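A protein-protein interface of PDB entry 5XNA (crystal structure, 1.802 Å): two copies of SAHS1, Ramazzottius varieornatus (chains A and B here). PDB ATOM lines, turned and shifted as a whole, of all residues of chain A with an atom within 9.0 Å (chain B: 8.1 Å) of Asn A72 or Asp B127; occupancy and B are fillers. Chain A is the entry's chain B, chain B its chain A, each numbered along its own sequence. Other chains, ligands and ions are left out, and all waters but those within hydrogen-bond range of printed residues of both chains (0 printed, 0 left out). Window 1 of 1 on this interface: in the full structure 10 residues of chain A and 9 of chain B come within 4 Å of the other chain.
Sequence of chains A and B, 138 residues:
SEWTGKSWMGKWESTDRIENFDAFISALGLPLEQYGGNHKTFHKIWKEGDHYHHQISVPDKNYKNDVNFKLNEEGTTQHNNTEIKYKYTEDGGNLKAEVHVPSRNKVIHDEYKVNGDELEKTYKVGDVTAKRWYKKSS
Of the printed residues of chain B, Asn A72 touches Asp B127.
Of the printed residues of chain B, Asp A91 touches Lys B124.
Leu A95 touches none of the printed residues of chain B.
Printed residues of chain B within 4 Å of Lys A96: Lys B124 (3.9 Å).
Printed residues of chain B within 4 Å of Glu A98: Val B107.
Of the printed residues of chain A, Val B107 touches Glu A98.
Of the printed residues of chain A, Asp B127 touches Asn A72 (3.1 Å).
No residue of chain A comes within 4 Å of Val B128.
Thr B129 touches none of the printed residues of chain A.
The nearest printed residue of chain B that does not touch Asn A72 is Gly B126 (5.4 Å).
The nearest printed residue of chain A that does not touch Asp B127 is Thr A89 (4.4 Å).
The backbone NH of Glu A98 is in hydrogen-bond range of the backbone carbonyl oxygen of Lys A87, at 2.9 Å.
The backbone carbonyl oxygen (O) of Thr A89 lies within hydrogen-bond range of the backbone NH (N) of Lys A96 (2.8 Å).
NZ of Lys A96 is in salt-bridge range of OD2 of Asp A91 (2.7 Å).
The backbone carbonyl oxygen of Tyr A88 is in hydrogen-bond range of the backbone NH of Asn A72 (2.8 Å).
Printed residues of chain B that touch a printed residue of chain A: Val B107, Lys B124 and Asp B127.
Hydrophobic or aromatic side chains of chain B within 4 Å of the printed part of chain A: Val B107.
Printed residues of chain A that touch a printed residue of chain B: Asn A72, Asp A91, Lys A96 and Glu A98.
OD2 of Asp A91 lies within salt-bridge range of NZ of Lys B124.
No position is printed for both chains.
Among the printed residues, merely in contact across the chains: Asn A72 with Asp B127 (3.1 Å), Lys A96 with Lys B124 (3.9 Å) and Glu A98 with Val B107 (3.8 Å).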
ATOM      1  N   ASP A  50     -26.584  16.189   6.756  1.00  0.00           N
ATOM      2  CA  ASP A  50     -27.406  15.852   5.609  1.00  0.00           C
ATOM      3  C   ASP A  50     -26.695  16.051   4.275  1.00  0.00           C
ATOM      4  O   ASP A  50     -27.312  15.830   3.223  1.00  0.00           O
ATOM      5  CB  ASP A  50     -28.713  16.670   5.650  1.00  0.00           C
ATOM      6  CG  ASP A  50     -28.490  18.206   5.763  1.00  0.00           C
ATOM      7  OD1 ASP A  50     -27.363  18.703   6.017  1.00  0.00           O
ATOM      8  OD2 ASP A  50     -29.496  18.935   5.604  1.00  0.00           O
ATOM      9  N   TYR A  52     -22.529  16.612   2.057  1.00  0.00           N
ATOM     10  CA  TYR A  52     -21.148  16.189   1.949  1.00  0.00           C
ATOM     11  C   TYR A  52     -20.251  17.380   1.679  1.00  0.00           C
ATOM     12  O   TYR A  52     -20.678  18.424   1.173  1.00  0.00           O
ATOM     13  CB  TYR A  52     -20.938  15.160   0.814  1.00  0.00           C
ATOM     14  CG  TYR A  52     -21.596  13.825   1.037  1.00  0.00           C
ATOM     15  CD1 TYR A  52     -22.925  13.616   0.678  1.00  0.00           C
ATOM     16  CD2 TYR A  52     -20.888  12.767   1.588  1.00  0.00           C
ATOM     17  CE1 TYR A  52     -23.539  12.392   0.884  1.00  0.00           C
ATOM     18  CE2 TYR A  52     -21.491  11.527   1.791  1.00  0.00           C
ATOM     19  CZ  TYR A  52     -22.815  11.355   1.434  1.00  0.00           C
ATOM     20  OH  TYR A  52     -23.420  10.145   1.625  1.00  0.00           O
ATOM     21  N   PHE A  69     -21.955  19.687  -1.070  1.00  0.00           N
ATOM     22  CA  PHE A  69     -22.965  19.141  -1.969  1.00  0.00           C
ATOM     23  C   PHE A  69     -23.935  18.234  -1.233  1.00  0.00           C
ATOM     24  O   PHE A  69     -23.564  17.515  -0.301  1.00  0.00           O
ATOM     25  CB  PHE A  69     -22.330  18.401  -3.177  1.00  0.00           C
ATOM     26  CG  PHE A  69     -21.671  17.059  -2.868  1.00  0.00           C
ATOM     27  CD1 PHE A  69     -22.406  15.892  -2.870  1.00  0.00           C
ATOM     28  CD2 PHE A  69     -20.301  16.966  -2.708  1.00  0.00           C
ATOM     29  CE1 PHE A  69     -21.799  14.665  -2.663  1.00  0.00           C
ATOM     30  CE2 PHE A  69     -19.678  15.741  -2.516  1.00  0.00           C
ATOM     31  CZ  PHE A  69     -20.426  14.588  -2.490  1.00  0.00           C
ATOM     32  N   LYS A  70     -25.192  18.278  -1.676  1.00  0.00           N
ATOM     33  CA  LYS A  70     -26.187  17.264  -1.358  1.00  0.00           C
ATOM     34  C   LYS A  70     -26.414  16.429  -2.601  1.00  0.00           C
ATOM     35  O   LYS A  70     -26.583  16.987  -3.690  1.00  0.00           O
ATOM     36  CB  LYS A  70     -27.522  17.880  -0.932  1.00  0.00           C
ATOM     37  CG  LYS A  70     -27.568  18.360   0.497  1.00  0.00           C
ATOM     38  CD  LYS A  70     -28.981  18.811   0.861  1.00  0.00           C
ATOM     39  CE  LYS A  70     -28.970  19.642   2.143  1.00  0.00           C
ATOM     40  NZ  LYS A  70     -30.343  20.034   2.576  1.00  0.00           N
ATOM     41  N   LEU A  71     -26.444  15.112  -2.441  1.00  0.00           N
ATOM     42  CA  LEU A  71     -26.637  14.255  -3.604  1.00  0.00           C
ATOM     43  C   LEU A  71     -27.938  14.626  -4.310  1.00  0.00           C
ATOM     44  O   LEU A  71     -28.965  14.826  -3.662  1.00  0.00           O
ATOM     45  CB  LEU A  71     -26.628  12.785  -3.186  1.00  0.00           C
ATOM     46  CG  LEU A  71     -25.229  12.264  -2.834  1.00  0.00           C
ATOM     47  CD1 LEU A  71     -25.273  10.924  -2.138  1.00  0.00           C
ATOM     48  CD2 LEU A  71     -24.357  12.146  -4.094  1.00  0.00           C
ATOM     49  N   ASN A  72     -27.861  14.779  -5.634  1.00  0.00           N
ATOM     50  CA  ASN A  72     -28.990  15.057  -6.521  1.00  0.00           C
ATOM     51  C   ASN A  72     -29.482  16.499  -6.458  1.00  0.00           C
ATOM     52  O   ASN A  72     -30.517  16.813  -7.065  1.00  0.00           O
ATOM     53  CB  ASN A  72     -30.157  14.101  -6.245  1.00  0.00           C
ATOM     54  CG  ASN A  72     -29.694  12.676  -6.092  1.00  0.00           C
ATOM     55  OD1 ASN A  72     -28.898  12.194  -6.888  1.00  0.00           O
ATOM     56  ND2 ASN A  72     -30.159  12.003  -5.045  1.00  0.00           N
ATOM     57  N   GLU A  73     -28.773  17.387  -5.765  1.00  0.00           N
ATOM     58  CA  GLU A  73     -29.184  18.776  -5.613  1.00  0.00           C
ATOM     59  C   GLU A  73     -28.152  19.689  -6.260  1.00  0.00           C
ATOM     60  O   GLU A  73     -26.961  19.588  -5.971  1.00  0.00           O
ATOM     61  CB  GLU A  73     -29.367  19.136  -4.134  1.00  0.00           C
ATOM     62  CG  GLU A  73     -30.486  18.355  -3.487  1.00  0.00           C
ATOM     63  CD  GLU A  73     -31.033  19.041  -2.250  1.00  0.00           C
ATOM     64  OE1 GLU A  73     -30.651  20.207  -1.997  1.00  0.00           O
ATOM     65  OE2 GLU A  73     -31.838  18.409  -1.534  1.00  0.00           O
ATOM     66  N   GLU A  74     -28.614  20.578  -7.142  1.00  0.00           N
ATOM     67  CA  GLU A  74     -27.710  21.531  -7.772  1.00  0.00           C
ATOM     68  C   GLU A  74     -27.067  22.448  -6.743  1.00  0.00           C
ATOM     69  O   GLU A  74     -27.740  22.975  -5.845  1.00  0.00           O
ATOM     70  CB  GLU A  74     -28.457  22.367  -8.818  1.00  0.00           C
ATOM     71  CG  GLU A  74     -27.542  23.315  -9.608  1.00  0.00           C
ATOM     72  CD  GLU A  74     -28.260  24.036 -10.744  1.00  0.00           C
ATOM     73  OE1 GLU A  74     -29.359  24.585 -10.528  1.00  0.00           O
ATOM     74  OE2 GLU A  74     -27.722  24.047 -11.864  1.00  0.00           O
ATOM     75  N   GLY A  75     -25.753  22.648  -6.881  1.00  0.00           N
ATOM     76  CA  GLY A  75     -25.026  23.627  -6.106  1.00  0.00           C
ATOM     77  C   GLY A  75     -24.308  24.610  -7.024  1.00  0.00           C
ATOM     78  O   GLY A  75     -24.244  24.430  -8.252  1.00  0.00           O
ATOM     79  N   TYR A  86     -22.992  22.747 -10.333  1.00  0.00           N
ATOM     80  CA  TYR A  86     -22.654  21.331 -10.260  1.00  0.00           C
ATOM     81  C   TYR A  86     -23.775  20.525  -9.614  1.00  0.00           C
ATOM     82  O   TYR A  86     -24.605  21.045  -8.861  1.00  0.00           O
ATOM     83  CB  TYR A  86     -21.353  21.090  -9.485  1.00  0.00           C
ATOM     84  CG  TYR A  86     -21.415  21.631  -8.069  1.00  0.00           C
ATOM     85  CD1 TYR A  86     -21.984  20.886  -7.031  1.00  0.00           C
ATOM     86  CD2 TYR A  86     -20.963  22.918  -7.783  1.00  0.00           C
ATOM     87  CE1 TYR A  86     -22.073  21.409  -5.733  1.00  0.00           C
ATOM     88  CE2 TYR A  86     -21.053  23.446  -6.487  1.00  0.00           C
ATOM     89  CZ  TYR A  86     -21.600  22.689  -5.475  1.00  0.00           C
ATOM     90  OH  TYR A  86     -21.666  23.227  -4.196  1.00  0.00           O
ATOM     91  N   LYS A  87     -23.765  19.229  -9.897  1.00  0.00           N
ATOM     92  CA  LYS A  87     -24.655  18.312  -9.197  1.00  0.00           C
ATOM     93  C   LYS A  87     -23.966  16.962  -9.091  1.00  0.00           C
ATOM     94  O   LYS A  87     -23.636  16.349 -10.114  1.00  0.00           O
ATOM     95  CB  LYS A  87     -26.001  18.179  -9.913  1.00  0.00           C
ATOM     96  CG  LYS A  87     -26.997  17.295  -9.173  1.00  0.00           C
ATOM     97  CD  LYS A  87     -28.254  17.058 -10.015  1.00  0.00           C
ATOM     98  CE  LYS A  87     -29.137  18.303 -10.078  1.00  0.00           C
ATOM     99  NZ  LYS A  87     -30.280  18.083 -11.040  1.00  0.00           N
ATOM    100  N   TYR A  88     -23.785  16.491  -7.861  1.00  0.00           N
ATOM    101  CA  TYR A  88     -23.243  15.166  -7.608  1.00  0.00           C
ATOM    102  C   TYR A  88     -24.378  14.160  -7.488  1.00  0.00           C
ATOM    103  O   TYR A  88     -25.422  14.459  -6.904  1.00  0.00           O
ATOM    104  CB  TYR A  88     -22.447  15.140  -6.302  1.00  0.00           C
ATOM    105  CG  TYR A  88     -21.129  15.873  -6.316  1.00  0.00           C
ATOM    106  CD1 TYR A  88     -21.078  17.260  -6.259  1.00  0.00           C
ATOM    107  CD2 TYR A  88     -19.940  15.170  -6.305  1.00  0.00           C
ATOM    108  CE1 TYR A  88     -19.851  17.932  -6.244  1.00  0.00           C
ATOM    109  CE2 TYR A  88     -18.710  15.829  -6.267  1.00  0.00           C
ATOM    110  CZ  TYR A  88     -18.680  17.201  -6.237  1.00  0.00           C
ATOM    111  OH  TYR A  88     -17.457  17.836  -6.209  1.00  0.00           O
ATOM    112  N   THR A  89     -24.152  12.961  -8.014  1.00  0.00           N
ATOM    113  CA  THR A  89     -25.130  11.878  -7.968  1.00  0.00           C
ATOM    114  C   THR A  89     -24.364  10.583  -7.769  1.00  0.00           C
ATOM    115  O   THR A  89     -23.147  10.528  -7.953  1.00  0.00           O
ATOM    116  CB  THR A  89     -25.982  11.765  -9.249  1.00  0.00           C
ATOM    117  OG1 THR A  89     -25.134  11.505 -10.380  1.00  0.00           O
ATOM    118  CG2 THR A  89     -26.778  13.041  -9.511  1.00  0.00           C
ATOM    119  N   GLU A  90     -25.085   9.541  -7.373  1.00  0.00           N
ATOM    120  CA  GLU A  90     -24.540   8.193  -7.371  1.00  0.00           C
ATOM    121  C   GLU A  90     -25.175   7.453  -8.522  1.00  0.00           C
ATOM    122  O   GLU A  90     -26.402   7.481  -8.688  1.00  0.00           O
ATOM    123  CB  GLU A  90     -24.820   7.450  -6.070  1.00  0.00           C
ATOM    124  CG  GLU A  90     -24.156   8.053  -4.892  1.00  0.00           C
ATOM    125  CD  GLU A  90     -24.388   7.232  -3.655  1.00  0.00           C
ATOM    126  OE1 GLU A  90     -25.511   7.306  -3.113  1.00  0.00           O
ATOM    127  OE2 GLU A  90     -23.459   6.501  -3.255  1.00  0.00           O
ATOM    128  N   ASP A  91     -24.349   6.786  -9.309  1.00  0.00           N
ATOM    129  CA  ASP A  91     -24.831   6.087 -10.487  1.00  0.00           C
ATOM    130  C   ASP A  91     -24.021   4.815 -10.622  1.00  0.00           C
ATOM    131  O   ASP A  91     -22.797   4.875 -10.763  1.00  0.00           O
ATOM    132  CB  ASP A  91     -24.694   6.967 -11.728  1.00  0.00           C
ATOM    133  CG  ASP A  91     -25.307   6.336 -12.966  1.00  0.00           C
ATOM    134  OD1 ASP A  91     -26.356   5.671 -12.833  1.00  0.00           O
ATOM    135  OD2 ASP A  91     -24.740   6.513 -14.068  1.00  0.00           O
ATOM    136  N   GLY A  92     -24.694   3.673 -10.562  1.00  0.00           N
ATOM    137  CA  GLY A  92     -23.977   2.411 -10.567  1.00  0.00           C
ATOM    138  C   GLY A  92     -23.033   2.262  -9.396  1.00  0.00           C
ATOM    139  O   GLY A  92     -22.034   1.545  -9.497  1.00  0.00           O
ATOM    140  N   LEU A  95     -19.558   7.632  -7.649  1.00  0.00           N
ATOM    141  CA  LEU A  95     -19.901   9.040  -7.495  1.00  0.00           C
ATOM    142  C   LEU A  95     -19.674   9.740  -8.827  1.00  0.00           C
ATOM    143  O   LEU A  95     -18.634   9.542  -9.457  1.00  0.00           O
ATOM    144  CB  LEU A  95     -19.043   9.693  -6.430  1.00  0.00           C
ATOM    145  CG  LEU A  95     -19.332  11.152  -6.088  1.00  0.00           C
ATOM    146  CD1 LEU A  95     -20.704  11.282  -5.439  1.00  0.00           C
ATOM    147  CD2 LEU A  95     -18.259  11.672  -5.147  1.00  0.00           C
ATOM    148  N   LYS A  96     -20.639  10.544  -9.255  1.00  0.00           N
ATOM    149  CA  LYS A  96     -20.511  11.341 -10.470  1.00  0.00           C
ATOM    150  C   LYS A  96     -20.726  12.810 -10.155  1.00  0.00           C
ATOM    151  O   LYS A  96     -21.524  13.154  -9.290  1.00  0.00           O
ATOM    152  CB  LYS A  96     -21.526  10.907 -11.523  1.00  0.00           C
ATOM    153  CG  LYS A  96     -21.219   9.567 -12.150  1.00  0.00           C
ATOM    154  CD  LYS A  96     -22.214   9.288 -13.290  1.00  0.00           C
ATOM    155  CE  LYS A  96     -21.780   8.061 -14.086  1.00  0.00           C
ATOM    156  NZ  LYS A  96     -22.662   7.814 -15.257  1.00  0.00           N
ATOM    157  N   GLU A  98     -21.712  16.366 -12.227  1.00  0.00           N
ATOM    158  CA  GLU A  98     -22.154  17.054 -13.439  1.00  0.00           C
ATOM    159  C   GLU A  98     -21.765  18.510 -13.256  1.00  0.00           C
ATOM    160  O   GLU A  98     -22.271  19.165 -12.347  1.00  0.00           O
ATOM    161  CB  GLU A  98     -23.664  16.911 -13.580  1.00  0.00           C
ATOM    162  CG  GLU A  98     -24.256  17.594 -14.803  1.00  0.00           C
ATOM    163  CD  GLU A  98     -24.070  16.765 -16.056  1.00  0.00           C
ATOM    164  OE1 GLU A  98     -23.755  15.556 -15.947  1.00  0.00           O
ATOM    165  OE2 GLU A  98     -24.242  17.342 -17.143  1.00  0.00           O
ATOM    166  N   ASN B  20     -38.745   2.154 -16.433  1.00  0.00           N
ATOM    167  CA  ASN B  20     -38.719   3.337 -15.570  1.00  0.00           C
ATOM    168  C   ASN B  20     -38.978   4.622 -16.345  1.00  0.00           C
ATOM    169  O   ASN B  20     -38.564   5.706 -15.921  1.00  0.00           O
ATOM    170  CB  ASN B  20     -37.392   3.443 -14.803  1.00  0.00           C
ATOM    171  CG  ASN B  20     -37.513   4.285 -13.533  1.00  0.00           C
ATOM    172  OD1 ASN B  20     -38.580   4.351 -12.920  1.00  0.00           O
ATOM    173  ND2 ASN B  20     -36.415   4.926 -13.132  1.00  0.00           N
ATOM    174  N   PHE B  24     -38.962   8.966 -15.478  1.00  0.00           N
ATOM    175  CA  PHE B  24     -38.153   9.937 -16.206  1.00  0.00           C
ATOM    176  C   PHE B  24     -39.007  11.104 -16.681  1.00  0.00           C
ATOM    177  O   PHE B  24     -38.641  12.271 -16.501  1.00  0.00           O
ATOM    178  CB  PHE B  24     -37.456   9.269 -17.390  1.00  0.00           C
ATOM    179  CG  PHE B  24     -36.817  10.251 -18.344  1.00  0.00           C
ATOM    180  CD1 PHE B  24     -35.600  10.852 -18.031  1.00  0.00           C
ATOM    181  CD2 PHE B  24     -37.433  10.576 -19.551  1.00  0.00           C
ATOM    182  CE1 PHE B  24     -35.008  11.757 -18.905  1.00  0.00           C
ATOM    183  CE2 PHE B  24     -36.846  11.477 -20.432  1.00  0.00           C
ATOM    184  CZ  PHE B  24     -35.638  12.068 -20.110  1.00  0.00           C
ATOM    185  N   ALA B  27     -39.955  13.269 -13.691  1.00  0.00           N
ATOM    186  CA  ALA B  27     -38.846  14.100 -13.228  1.00  0.00           C
ATOM    187  C   ALA B  27     -38.626  15.304 -14.135  1.00  0.00           C
ATOM    188  O   ALA B  27     -38.087  16.326 -13.692  1.00  0.00           O
ATOM    189  CB  ALA B  27     -37.573  13.262 -13.134  1.00  0.00           C
ATOM    190  N   VAL B 107     -31.089  19.517 -17.374  1.00  0.00           N
ATOM    191  CA  VAL B 107     -30.072  18.922 -18.243  1.00  0.00           C
ATOM    192  C   VAL B 107     -30.426  17.453 -18.430  1.00  0.00           C
ATOM    193  O   VAL B 107     -30.559  16.711 -17.449  1.00  0.00           O
ATOM    194  CB  VAL B 107     -28.660  19.073 -17.659  1.00  0.00           C
ATOM    195  CG1 VAL B 107     -27.647  18.347 -18.562  1.00  0.00           C
ATOM    196  CG2 VAL B 107     -28.286  20.554 -17.493  1.00  0.00           C
ATOM    197  N   TYR B 123     -32.199   7.383 -20.968  1.00  0.00           N
ATOM    198  CA  TYR B 123     -32.598   8.759 -20.706  1.00  0.00           C
ATOM    199  C   TYR B 123     -32.282   9.064 -19.247  1.00  0.00           C
ATOM    200  O   TYR B 123     -32.687   8.308 -18.361  1.00  0.00           O
ATOM    201  CB  TYR B 123     -34.096   8.962 -20.947  1.00  0.00           C
ATOM    202  CG  TYR B 123     -34.692   8.339 -22.203  1.00  0.00           C
ATOM    203  CD1 TYR B 123     -34.762   6.950 -22.366  1.00  0.00           C
ATOM    204  CD2 TYR B 123     -35.266   9.136 -23.182  1.00  0.00           C
ATOM    205  CE1 TYR B 123     -35.337   6.381 -23.496  1.00  0.00           C
ATOM    206  CE2 TYR B 123     -35.848   8.576 -24.315  1.00  0.00           C
ATOM    207  CZ  TYR B 123     -35.881   7.201 -24.468  1.00  0.00           C
ATOM    208  OH  TYR B 123     -36.460   6.651 -25.595  1.00  0.00           O
ATOM    209  N   LYS B 124     -31.597  10.178 -18.981  1.00  0.00           N
ATOM    210  CA  LYS B 124     -31.196  10.459 -17.608  1.00  0.00           C
ATOM    211  C   LYS B 124     -31.301  11.941 -17.304  1.00  0.00           C
ATOM    212  O   LYS B 124     -30.749  12.768 -18.035  1.00  0.00           O
ATOM    213  CB  LYS B 124     -29.765   9.973 -17.345  1.00  0.00           C
ATOM    214  CG  LYS B 124     -29.362   9.968 -15.882  1.00  0.00           C
ATOM    215  CD  LYS B 124     -27.960   9.404 -15.712  1.00  0.00           C
ATOM    216  CE  LYS B 124     -27.794   8.100 -16.476  1.00  0.00           C
ATOM    217  NZ  LYS B 124     -26.415   7.541 -16.368  1.00  0.00           N
ATOM    218  N   VAL B 125     -31.986  12.274 -16.208  1.00  0.00           N
ATOM    219  CA  VAL B 125     -32.111  13.655 -15.763  1.00  0.00           C
ATOM    220  C   VAL B 125     -31.871  13.634 -14.263  1.00  0.00           C
ATOM    221  O   VAL B 125     -32.565  12.923 -13.529  1.00  0.00           O
ATOM    222  CB  VAL B 125     -33.468  14.280 -16.140  1.00  0.00           C
ATOM    223  CG1 VAL B 125     -34.677  13.470 -15.600  1.00  0.00           C
ATOM    224  CG2 VAL B 125     -33.519  15.763 -15.758  1.00  0.00           C
ATOM    225  N   GLY B 126     -30.827  14.326 -13.821  1.00  0.00           N
ATOM    226  CA  GLY B 126     -30.372  14.150 -12.450  1.00  0.00           C
ATOM    227  C   GLY B 126     -30.142  12.690 -12.108  1.00  0.00           C
ATOM    228  O   GLY B 126     -29.379  11.993 -12.785  1.00  0.00           O
ATOM    229  N   ASP B 127     -30.807  12.190 -11.067  1.00  0.00           N
ATOM    230  CA  ASP B 127     -30.601  10.819 -10.621  1.00  0.00           C
ATOM    231  C   ASP B 127     -31.656   9.850 -11.145  1.00  0.00           C
ATOM    232  O   ASP B 127     -31.722   8.714 -10.668  1.00  0.00           O
ATOM    233  CB  ASP B 127     -30.580  10.757  -9.091  1.00  0.00           C
ATOM    234  CG  ASP B 127     -31.917  11.105  -8.481  1.00  0.00           C
ATOM    235  OD1 ASP B 127     -32.609  12.002  -9.012  1.00  0.00           O
ATOM    236  OD2 ASP B 127     -32.293  10.481  -7.466  1.00  0.00           O
ATOM    237  N   VAL B 128     -32.485  10.264 -12.098  1.00  0.00           N
ATOM    238  CA  VAL B 128     -33.534   9.409 -12.643  1.00  0.00           C
ATOM    239  C   VAL B 128     -33.090   8.871 -13.993  1.00  0.00           C
ATOM    240  O   VAL B 128     -32.804   9.650 -14.904  1.00  0.00           O
ATOM    241  CB  VAL B 128     -34.858  10.174 -12.771  1.00  0.00           C
ATOM    242  CG1 VAL B 128     -35.951   9.258 -13.288  1.00  0.00           C
ATOM    243  CG2 VAL B 128     -35.234  10.797 -11.444  1.00  0.00           C
ATOM    244  N   THR B 129     -33.055   7.545 -14.128  1.00  0.00           N
ATOM    245  CA  THR B 129     -32.586   6.862 -15.329  1.00  0.00           C
ATOM    246  C   THR B 129     -33.720   6.034 -15.915  1.00  0.00           C
ATOM    247  O   THR B 129     -34.365   5.272 -15.190  1.00  0.00           O
ATOM    248  CB  THR B 129     -31.402   5.946 -15.012  1.00  0.00           C
ATOM    249  OG1 THR B 129     -30.313   6.723 -14.503  1.00  0.00           O
ATOM    250  CG2 THR B 129     -30.954   5.188 -16.261  1.00  0.00           C
ATOM    251  N   ALA B 130     -33.959   6.171 -17.221  1.00  0.00           N
ATOM    252  CA  ALA B 130     -34.904   5.301 -17.908  1.00  0.00           C
ATOM    253  C   ALA B 130     -34.239   4.661 -19.119  1.00  0.00           C
ATOM    254  O   ALA B 130     -33.205   5.114 -19.612  1.00  0.00           O
ATOM    255  CB  ALA B 130     -36.169   6.052 -18.337  1.00  0.00           C
